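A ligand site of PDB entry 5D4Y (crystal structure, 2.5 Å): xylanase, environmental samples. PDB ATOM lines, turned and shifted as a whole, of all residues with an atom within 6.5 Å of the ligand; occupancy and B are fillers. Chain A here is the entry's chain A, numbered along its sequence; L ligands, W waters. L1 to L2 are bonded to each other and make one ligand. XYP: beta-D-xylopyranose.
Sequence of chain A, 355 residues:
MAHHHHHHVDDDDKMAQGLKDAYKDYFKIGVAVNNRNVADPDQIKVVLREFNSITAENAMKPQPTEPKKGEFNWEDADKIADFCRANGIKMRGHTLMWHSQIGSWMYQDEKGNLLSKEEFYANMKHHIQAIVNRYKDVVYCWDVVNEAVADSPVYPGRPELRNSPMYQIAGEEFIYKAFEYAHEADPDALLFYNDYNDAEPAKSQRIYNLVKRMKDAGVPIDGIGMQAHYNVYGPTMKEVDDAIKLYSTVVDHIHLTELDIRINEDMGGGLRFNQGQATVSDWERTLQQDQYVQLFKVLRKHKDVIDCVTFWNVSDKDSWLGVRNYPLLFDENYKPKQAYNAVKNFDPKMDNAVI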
ATOM      1  N   ALA A  56     -18.303  16.691 -26.310  1.00  0.00           N
ATOM      2  CA  ALA A  56     -16.907  17.053 -25.852  1.00  0.00           C
ATOM      3  C   ALA A  56     -16.953  18.421 -25.188  1.00  0.00           C
ATOM      4  O   ALA A  56     -17.383  19.386 -25.788  1.00  0.00           O
ATOM      5  CB  ALA A  56     -15.888  17.044 -26.996  1.00  0.00           C
ATOM      6  N   GLU A  57     -16.592  18.503 -23.923  1.00  0.00           N
ATOM      7  CA  GLU A  57     -16.527  19.800 -23.295  1.00  0.00           C
ATOM      8  C   GLU A  57     -15.594  20.762 -24.070  1.00  0.00           C
ATOM      9  O   GLU A  57     -15.945  21.933 -24.242  1.00  0.00           O
ATOM     10  CB  GLU A  57     -16.124  19.685 -21.814  1.00  0.00           C
ATOM     11  CG  GLU A  57     -15.465  20.948 -21.301  1.00  0.00           C
ATOM     12  CD  GLU A  57     -15.292  20.974 -19.797  1.00  0.00           C
ATOM     13  OE1 GLU A  57     -14.836  19.964 -19.202  1.00  0.00           O
ATOM     14  OE2 GLU A  57     -15.598  22.045 -19.225  1.00  0.00           O
ATOM     15  N   ASN A  58     -14.448  20.275 -24.545  1.00  0.00           N
ATOM     16  CA  ASN A  58     -13.461  21.153 -25.278  1.00  0.00           C
ATOM     17  C   ASN A  58     -12.849  20.650 -26.592  1.00  0.00           C
ATOM     18  O   ASN A  58     -12.438  21.476 -27.445  1.00  0.00           O
ATOM     19  CB  ASN A  58     -12.277  21.508 -24.363  1.00  0.00           C
ATOM     20  CG  ASN A  58     -12.637  22.547 -23.324  1.00  0.00           C
ATOM     21  OD1 ASN A  58     -12.679  22.269 -22.120  1.00  0.00           O
ATOM     22  ND2 ASN A  58     -12.906  23.746 -23.781  1.00  0.00           N
ATOM     23  N   LYS A  61     -13.808  21.996 -30.189  1.00  0.00           N
ATOM     24  CA  LYS A  61     -13.824  23.412 -30.449  1.00  0.00           C
ATOM     25  C   LYS A  61     -12.709  23.816 -31.449  1.00  0.00           C
ATOM     26  O   LYS A  61     -11.734  23.101 -31.606  1.00  0.00           O
ATOM     27  CB  LYS A  61     -13.689  24.189 -29.165  1.00  0.00           C
ATOM     28  CG  LYS A  61     -14.930  24.175 -28.319  1.00  0.00           C
ATOM     29  CD  LYS A  61     -14.646  24.852 -26.993  1.00  0.00           C
ATOM     30  CE  LYS A  61     -15.837  24.782 -26.055  1.00  0.00           C
ATOM     31  NZ  LYS A  61     -15.446  24.733 -24.623  1.00  0.00           N
ATOM     32  N   HIS A  94     -19.811  19.652 -30.403  1.00  0.00           N
ATOM     33  CA  HIS A  94     -19.765  21.010 -29.917  1.00  0.00           C
ATOM     34  C   HIS A  94     -18.469  21.690 -30.367  1.00  0.00           C
ATOM     35  O   HIS A  94     -17.371  21.112 -30.324  1.00  0.00           O
ATOM     36  CB  HIS A  94     -19.996  21.021 -28.420  1.00  0.00           C
ATOM     37  CG  HIS A  94     -20.242  22.399 -27.873  1.00  0.00           C
ATOM     38  ND1 HIS A  94     -19.257  23.129 -27.251  1.00  0.00           N
ATOM     39  CD2 HIS A  94     -21.356  23.156 -27.856  1.00  0.00           C
ATOM     40  CE1 HIS A  94     -19.763  24.291 -26.856  1.00  0.00           C
ATOM     41  NE2 HIS A  94     -21.032  24.332 -27.213  1.00  0.00           N
ATOM     42  N   THR A  95     -18.599  23.004 -30.452  1.00  0.00           N
ATOM     43  CA  THR A  95     -18.936  23.750 -31.686  1.00  0.00           C
ATOM     44  C   THR A  95     -17.967  24.035 -32.844  1.00  0.00           C
ATOM     45  O   THR A  95     -16.772  24.162 -32.634  1.00  0.00           O
ATOM     46  CB  THR A  95     -19.541  25.081 -31.207  1.00  0.00           C
ATOM     47  OG1 THR A  95     -20.310  25.695 -32.237  1.00  0.00           O
ATOM     48  CG2 THR A  95     -18.436  25.991 -30.706  1.00  0.00           C
ATOM     49  N   TRP A  98     -17.438  29.821 -33.289  1.00  0.00           N
ATOM     50  CA  TRP A  98     -17.636  30.544 -32.040  1.00  0.00           C
ATOM     51  C   TRP A  98     -16.584  31.652 -31.899  1.00  0.00           C
ATOM     52  O   TRP A  98     -15.451  31.516 -32.358  1.00  0.00           O
ATOM     53  CB  TRP A  98     -17.501  29.543 -30.888  1.00  0.00           C
ATOM     54  CG  TRP A  98     -17.839  30.070 -29.580  1.00  0.00           C
ATOM     55  CD1 TRP A  98     -18.702  31.052 -29.321  1.00  0.00           C
ATOM     56  CD2 TRP A  98     -17.362  29.609 -28.325  1.00  0.00           C
ATOM     57  NE1 TRP A  98     -18.783  31.265 -27.970  1.00  0.00           N
ATOM     58  CE2 TRP A  98     -17.975  30.364 -27.336  1.00  0.00           C
ATOM     59  CE3 TRP A  98     -16.492  28.613 -27.950  1.00  0.00           C
ATOM     60  CZ2 TRP A  98     -17.729  30.179 -25.990  1.00  0.00           C
ATOM     61  CZ3 TRP A  98     -16.257  28.422 -26.613  1.00  0.00           C
ATOM     62  CH2 TRP A  98     -16.870  29.204 -25.651  1.00  0.00           C
ATOM     63  N   GLN A 101     -12.578  30.294 -27.847  1.00  0.00           N
ATOM     64  CA  GLN A 101     -11.725  29.148 -28.155  1.00  0.00           C
ATOM     65  C   GLN A 101     -11.549  28.944 -29.629  1.00  0.00           C
ATOM     66  O   GLN A 101     -11.765  27.862 -30.159  1.00  0.00           O
ATOM     67  CB  GLN A 101     -12.184  27.904 -27.408  1.00  0.00           C
ATOM     68  CG  GLN A 101     -12.053  28.130 -25.907  1.00  0.00           C
ATOM     69  CD  GLN A 101     -12.430  26.933 -25.049  1.00  0.00           C
ATOM     70  OE1 GLN A 101     -11.683  25.968 -24.972  1.00  0.00           O
ATOM     71  NE2 GLN A 101     -13.572  27.041 -24.360  1.00  0.00           N
ATOM     72  N   ASN A 146     -22.293  29.365 -32.341  1.00  0.00           N
ATOM     73  CA  ASN A 146     -22.402  29.426 -30.915  1.00  0.00           C
ATOM     74  C   ASN A 146     -22.410  30.889 -30.520  1.00  0.00           C
ATOM     75  O   ASN A 146     -21.545  31.626 -30.912  1.00  0.00           O
ATOM     76  CB  ASN A 146     -21.158  28.739 -30.320  1.00  0.00           C
ATOM     77  CG  ASN A 146     -21.373  28.199 -28.942  1.00  0.00           C
ATOM     78  OD1 ASN A 146     -22.441  27.633 -28.636  1.00  0.00           O
ATOM     79  ND2 ASN A 146     -20.350  28.348 -28.081  1.00  0.00           N
ATOM     80  N   GLU A 147     -23.394  31.331 -29.763  1.00  0.00           N
ATOM     81  CA  GLU A 147     -23.327  32.608 -29.054  1.00  0.00           C
ATOM     82  C   GLU A 147     -23.154  33.795 -29.989  1.00  0.00           C
ATOM     83  O   GLU A 147     -22.387  34.716 -29.711  1.00  0.00           O
ATOM     84  CB  GLU A 147     -22.226  32.570 -27.964  1.00  0.00           C
ATOM     85  CG  GLU A 147     -22.340  31.344 -27.044  1.00  0.00           C
ATOM     86  CD  GLU A 147     -21.367  31.330 -25.847  1.00  0.00           C
ATOM     87  OE1 GLU A 147     -20.327  32.067 -25.847  1.00  0.00           O
ATOM     88  OE2 GLU A 147     -21.633  30.539 -24.894  1.00  0.00           O
ATOM     89  N   ASN A 194     -26.938  27.610 -31.224  1.00  0.00           N
ATOM     90  CA  ASN A 194     -26.769  27.356 -29.804  1.00  0.00           C
ATOM     91  C   ASN A 194     -26.531  28.682 -29.106  1.00  0.00           C
ATOM     92  O   ASN A 194     -25.719  29.480 -29.578  1.00  0.00           O
ATOM     93  CB  ASN A 194     -25.549  26.453 -29.604  1.00  0.00           C
ATOM     94  CG  ASN A 194     -25.427  25.898 -28.215  1.00  0.00           C
ATOM     95  OD1 ASN A 194     -24.348  25.897 -27.622  1.00  0.00           O
ATOM     96  ND2 ASN A 194     -26.536  25.396 -27.693  1.00  0.00           N
ATOM     97  N   TYR A 196     -26.894  31.024 -25.005  1.00  0.00           N
ATOM     98  CA  TYR A 196     -27.174  31.158 -23.565  1.00  0.00           C
ATOM     99  C   TYR A 196     -28.080  32.350 -23.339  1.00  0.00           C
ATOM    100  O   TYR A 196     -28.256  33.168 -24.215  1.00  0.00           O
ATOM    101  CB  TYR A 196     -25.871  31.331 -22.763  1.00  0.00           C
ATOM    102  CG  TYR A 196     -25.122  32.653 -22.957  1.00  0.00           C
ATOM    103  CD1 TYR A 196     -25.484  33.790 -22.271  1.00  0.00           C
ATOM    104  CD2 TYR A 196     -24.057  32.739 -23.831  1.00  0.00           C
ATOM    105  CE1 TYR A 196     -24.807  34.967 -22.459  1.00  0.00           C
ATOM    106  CE2 TYR A 196     -23.376  33.925 -24.030  1.00  0.00           C
ATOM    107  CZ  TYR A 196     -23.759  35.026 -23.333  1.00  0.00           C
ATOM    108  OH  TYR A 196     -23.051  36.184 -23.513  1.00  0.00           O
ATOM    109  N   GLN A 227     -28.662  26.649 -23.988  1.00  0.00           N
ATOM    110  CA  GLN A 227     -27.528  26.275 -23.163  1.00  0.00           C
ATOM    111  C   GLN A 227     -28.013  25.885 -21.791  1.00  0.00           C
ATOM    112  O   GLN A 227     -27.594  24.868 -21.218  1.00  0.00           O
ATOM    113  CB  GLN A 227     -26.456  27.390 -23.123  1.00  0.00           C
ATOM    114  CG  GLN A 227     -25.460  27.165 -24.258  1.00  0.00           C
ATOM    115  CD  GLN A 227     -24.368  28.207 -24.450  1.00  0.00           C
ATOM    116  OE1 GLN A 227     -24.061  28.547 -25.575  1.00  0.00           O
ATOM    117  NE2 GLN A 227     -23.728  28.623 -23.389  1.00  0.00           N
ATOM    118  N   HIS A 229     -27.582  27.542 -18.965  1.00  0.00           N
ATOM    119  CA  HIS A 229     -26.794  27.986 -17.816  1.00  0.00           C
ATOM    120  C   HIS A 229     -27.677  28.820 -16.920  1.00  0.00           C
ATOM    121  O   HIS A 229     -27.605  30.042 -16.915  1.00  0.00           O
ATOM    122  CB  HIS A 229     -25.567  28.778 -18.246  1.00  0.00           C
ATOM    123  CG  HIS A 229     -24.553  27.936 -18.939  1.00  0.00           C
ATOM    124  ND1 HIS A 229     -23.976  26.834 -18.345  1.00  0.00           N
ATOM    125  CD2 HIS A 229     -24.100  27.967 -20.209  1.00  0.00           C
ATOM    126  CE1 HIS A 229     -23.189  26.236 -19.210  1.00  0.00           C
ATOM    127  NE2 HIS A 229     -23.250  26.896 -20.353  1.00  0.00           N
ATOM    128  N   THR A 257     -28.595  21.997 -23.725  1.00  0.00           N
ATOM    129  CA  THR A 257     -27.318  21.711 -24.288  1.00  0.00           C
ATOM    130  C   THR A 257     -26.156  21.725 -23.293  1.00  0.00           C
ATOM    131  O   THR A 257     -25.226  20.957 -23.446  1.00  0.00           O
ATOM    132  CB  THR A 257     -27.186  22.702 -25.418  1.00  0.00           C
ATOM    133  OG1 THR A 257     -27.410  22.019 -26.647  1.00  0.00           O
ATOM    134  CG2 THR A 257     -25.904  23.371 -25.462  1.00  0.00           C
ATOM    135  N   GLU A 258     -26.224  22.596 -22.290  1.00  0.00           N
ATOM    136  CA  GLU A 258     -25.160  22.783 -21.284  1.00  0.00           C
ATOM    137  C   GLU A 258     -25.793  23.077 -19.908  1.00  0.00           C
ATOM    138  O   GLU A 258     -25.453  24.043 -19.225  1.00  0.00           O
ATOM    139  CB  GLU A 258     -24.217  23.945 -21.685  1.00  0.00           C
ATOM    140  CG  GLU A 258     -23.880  23.939 -23.150  1.00  0.00           C
ATOM    141  CD  GLU A 258     -22.882  25.002 -23.596  1.00  0.00           C
ATOM    142  OE1 GLU A 258     -22.311  25.777 -22.765  1.00  0.00           O
ATOM    143  OE2 GLU A 258     -22.672  25.054 -24.841  1.00  0.00           O
ATOM    144  N   TRP A 312     -23.956  20.142 -18.388  1.00  0.00           N
ATOM    145  CA  TRP A 312     -22.680  20.598 -18.864  1.00  0.00           C
ATOM    146  C   TRP A 312     -21.488  19.810 -18.326  1.00  0.00           C
ATOM    147  O   TRP A 312     -20.568  19.578 -19.088  1.00  0.00           O
ATOM    148  CB  TRP A 312     -22.444  22.090 -18.667  1.00  0.00           C
ATOM    149  CG  TRP A 312     -21.252  22.521 -19.430  1.00  0.00           C
ATOM    150  CD1 TRP A 312     -20.178  23.172 -18.957  1.00  0.00           C
ATOM    151  CD2 TRP A 312     -20.977  22.264 -20.817  1.00  0.00           C
ATOM    152  NE1 TRP A 312     -19.248  23.377 -19.948  1.00  0.00           N
ATOM    153  CE2 TRP A 312     -19.724  22.837 -21.104  1.00  0.00           C
ATOM    154  CE3 TRP A 312     -21.673  21.616 -21.830  1.00  0.00           C
ATOM    155  CZ2 TRP A 312     -19.144  22.774 -22.357  1.00  0.00           C
ATOM    156  CZ3 TRP A 312     -21.100  21.546 -23.082  1.00  0.00           C
ATOM    157  CH2 TRP A 312     -19.854  22.130 -23.344  1.00  0.00           C
ATOM    158  N   ASN A 313     -21.437  19.373 -17.085  1.00  0.00           N
ATOM    159  CA  ASN A 313     -20.326  18.498 -16.719  1.00  0.00           C
ATOM    160  C   ASN A 313     -20.806  17.241 -16.011  1.00  0.00           C
ATOM    161  O   ASN A 313     -22.012  17.061 -15.781  1.00  0.00           O
ATOM    162  CB  ASN A 313     -19.295  19.259 -15.861  1.00  0.00           C
ATOM    163  CG  ASN A 313     -18.555  20.329 -16.653  1.00  0.00           C
ATOM    164  OD1 ASN A 313     -18.729  21.529 -16.437  1.00  0.00           O
ATOM    165  ND2 ASN A 313     -17.732  19.890 -17.594  1.00  0.00           N
ATOM    166  N   ASP A 318     -15.819  18.546 -11.780  1.00  0.00           N
ATOM    167  CA  ASP A 318     -15.345  19.015 -13.103  1.00  0.00           C
ATOM    168  C   ASP A 318     -16.197  20.160 -13.752  1.00  0.00           C
ATOM    169  O   ASP A 318     -15.906  20.595 -14.876  1.00  0.00           O
ATOM    170  CB  ASP A 318     -15.059  17.855 -14.099  1.00  0.00           C
ATOM    171  CG  ASP A 318     -15.952  16.605 -13.901  1.00  0.00           C
ATOM    172  OD1 ASP A 318     -17.174  16.711 -13.602  1.00  0.00           O
ATOM    173  OD2 ASP A 318     -15.398  15.484 -14.080  1.00  0.00           O
ATOM    174  N   TRP A 320     -17.162  23.665 -14.837  1.00  0.00           N
ATOM    175  CA  TRP A 320     -16.510  24.928 -15.236  1.00  0.00           C
ATOM    176  C   TRP A 320     -16.814  26.110 -14.325  1.00  0.00           C
ATOM    177  O   TRP A 320     -16.189  27.160 -14.446  1.00  0.00           O
ATOM    178  CB  TRP A 320     -16.934  25.303 -16.661  1.00  0.00           C
ATOM    179  CG  TRP A 320     -18.365  25.841 -16.833  1.00  0.00           C
ATOM    180  CD1 TRP A 320     -19.536  25.172 -16.578  1.00  0.00           C
ATOM    181  CD2 TRP A 320     -18.762  27.130 -17.361  1.00  0.00           C
ATOM    182  NE1 TRP A 320     -20.620  25.964 -16.893  1.00  0.00           N
ATOM    183  CE2 TRP A 320     -20.177  27.161 -17.378  1.00  0.00           C
ATOM    184  CE3 TRP A 320     -18.060  28.252 -17.812  1.00  0.00           C
ATOM    185  CZ2 TRP A 320     -20.887  28.286 -17.809  1.00  0.00           C
ATOM    186  CZ3 TRP A 320     -18.767  29.342 -18.251  1.00  0.00           C
ATOM    187  CH2 TRP A 320     -20.161  29.353 -18.246  1.00  0.00           C
HETATM  188  C1  XYP L   1     -13.107  26.397 -20.510  1.00  0.00           C
HETATM  189  C2  XYP L   1     -14.059  25.226 -20.045  1.00  0.00           C
HETATM  190  C3  XYP L   1     -15.313  25.067 -20.881  1.00  0.00           C
HETATM  191  C4  XYP L   1     -16.031  26.318 -21.147  1.00  0.00           C
HETATM  192  C5  XYP L   1     -15.095  27.543 -21.395  1.00  0.00           C
HETATM  193  O2  XYP L   1     -13.453  23.977 -20.179  1.00  0.00           O
HETATM  194  O3  XYP L   1     -16.243  24.243 -20.165  1.00  0.00           O
HETATM  195  O4  XYP L   1     -16.727  25.955 -22.278  1.00  0.00           O
HETATM  196  O5  XYP L   1     -13.708  27.094 -21.630  1.00  0.00           O
HETATM  197  C1  XYP L   2     -18.154  26.001 -22.383  1.00  0.00           C
HETATM  198  C2  XYP L   2     -18.727  27.470 -22.250  1.00  0.00           C
HETATM  199  C3  XYP L   2     -20.048  27.529 -23.056  1.00  0.00           C
HETATM  200  C4  XYP L   2     -19.707  27.425 -24.540  1.00  0.00           C
HETATM  201  C5  XYP L   2     -18.494  26.465 -24.753  1.00  0.00           C
HETATM  202  O2  XYP L   2     -19.011  27.761 -20.897  1.00  0.00           O
HETATM  203  O3  XYP L   2     -20.888  28.700 -22.779  1.00  0.00           O
HETATM  204  O4  XYP L   2     -20.851  26.968 -25.242  1.00  0.00           O
HETATM  205  O5  XYP L   2     -18.480  25.423 -23.763  1.00  0.00           O
HETATM  206  O   HOH W   1     -22.135  30.902 -21.940  1.00  0.00           O
HETATM  207  O   HOH W   2     -10.443  24.129 -20.384  1.00  0.00           O
HETATM  208  O   HOH W   3     -10.892  28.636 -22.087  1.00  0.00           O
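An oxygen (O4) of XYP L2 lies within hydrogen-bond range of the side-chain carboxylate (OE2) of Glu 258 (2.7 Å). An oxygen (O2) of XYP L1 is in hydrogen-bond range of the side-chain amide oxygen (OD1) of Asn 58. The side-chain amide nitrogen (NE2) of Gln 227 lies within hydrogen-bond range of an oxygen (O3) of XYP L2, at 2.9 Å. The side-chain amide nitrogen (ND2) of Asn 146 lies within hydrogen-bond range of an oxygen (O4) of XYP L2 (3.2 Å). An oxygen (O4) of XYP L2 sits at hydrogen-bond distance from a ring nitrogen (NE2) of His 94. An oxygen (O3) of XYP L2 is in hydrogen-bond range of the side-chain carboxylate (OE2) of Glu 147 (2.9 Å). O4 of XYP L1 sits at hydrogen-bond distance from NZ of Lys 61. O3 of XYP L1 is in hydrogen-bond range of OE2 of Glu 57 (2.5 Å). NE1 of Trp 312 is in hydrogen-bond range of O3 of XYP L1 (3.1 Å). An oxygen (O5) of XYP L1 is in hydrogen-bond range of the side-chain amide nitrogen of Gln 101, 2.7 Å away.
The side-chain amide nitrogen (ND2) of Asn 313 sits at hydrogen-bond distance from the side-chain carboxylate (OE1) of Glu 57 (3.3 Å). N of Glu 258 lies close to O of Gln 227, 2.9 Å away. The side-chain carboxylate (OE1) of Glu 147 sits at hydrogen-bond distance from the indole nitrogen (NE1) of Trp 98 (2.7 Å). OD1 of Asn 146 sits close to OD1 of Asn 194 (2.8 Å). N of Glu 147 sits at hydrogen-bond distance from O of Asn 194, at 3.0 Å. OE1 of Gln 101 sits at hydrogen-bond distance from ND2 of Asn 58 (2.8 Å). The side-chain carboxylate of Glu 147 is in hydrogen-bond range of the side-chain amide nitrogen of Gln 227, at 3.2 Å. The side-chain amino group (NZ) of Lys 61 sits at hydrogen-bond distance from the backbone carbonyl oxygen (O) of Glu 57, at 2.9 Å.
Merely in contact with the ligand: Trp 98 (3.3 Å), His 229 (3.8 Å) and Trp 320 (3.1 Å). 13 residues have an atom within 4 Å of the ligand: Glu 57, Asn 58, Lys 61, His 94, Trp 98, Gln 101, Asn 146, Glu 147, Gln 227, His 229, Glu 258, Trp 312 and Trp 320.
Water W1 lies within hydrogen-bond range of O3 of XYP L2 (2.7 Å), OE2 of Glu 147 (3.0 Å) and NE2 of Gln 227 (3.1 Å). Water W2 bridges O2 of XYP L1 and OD1 of Asn 58.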
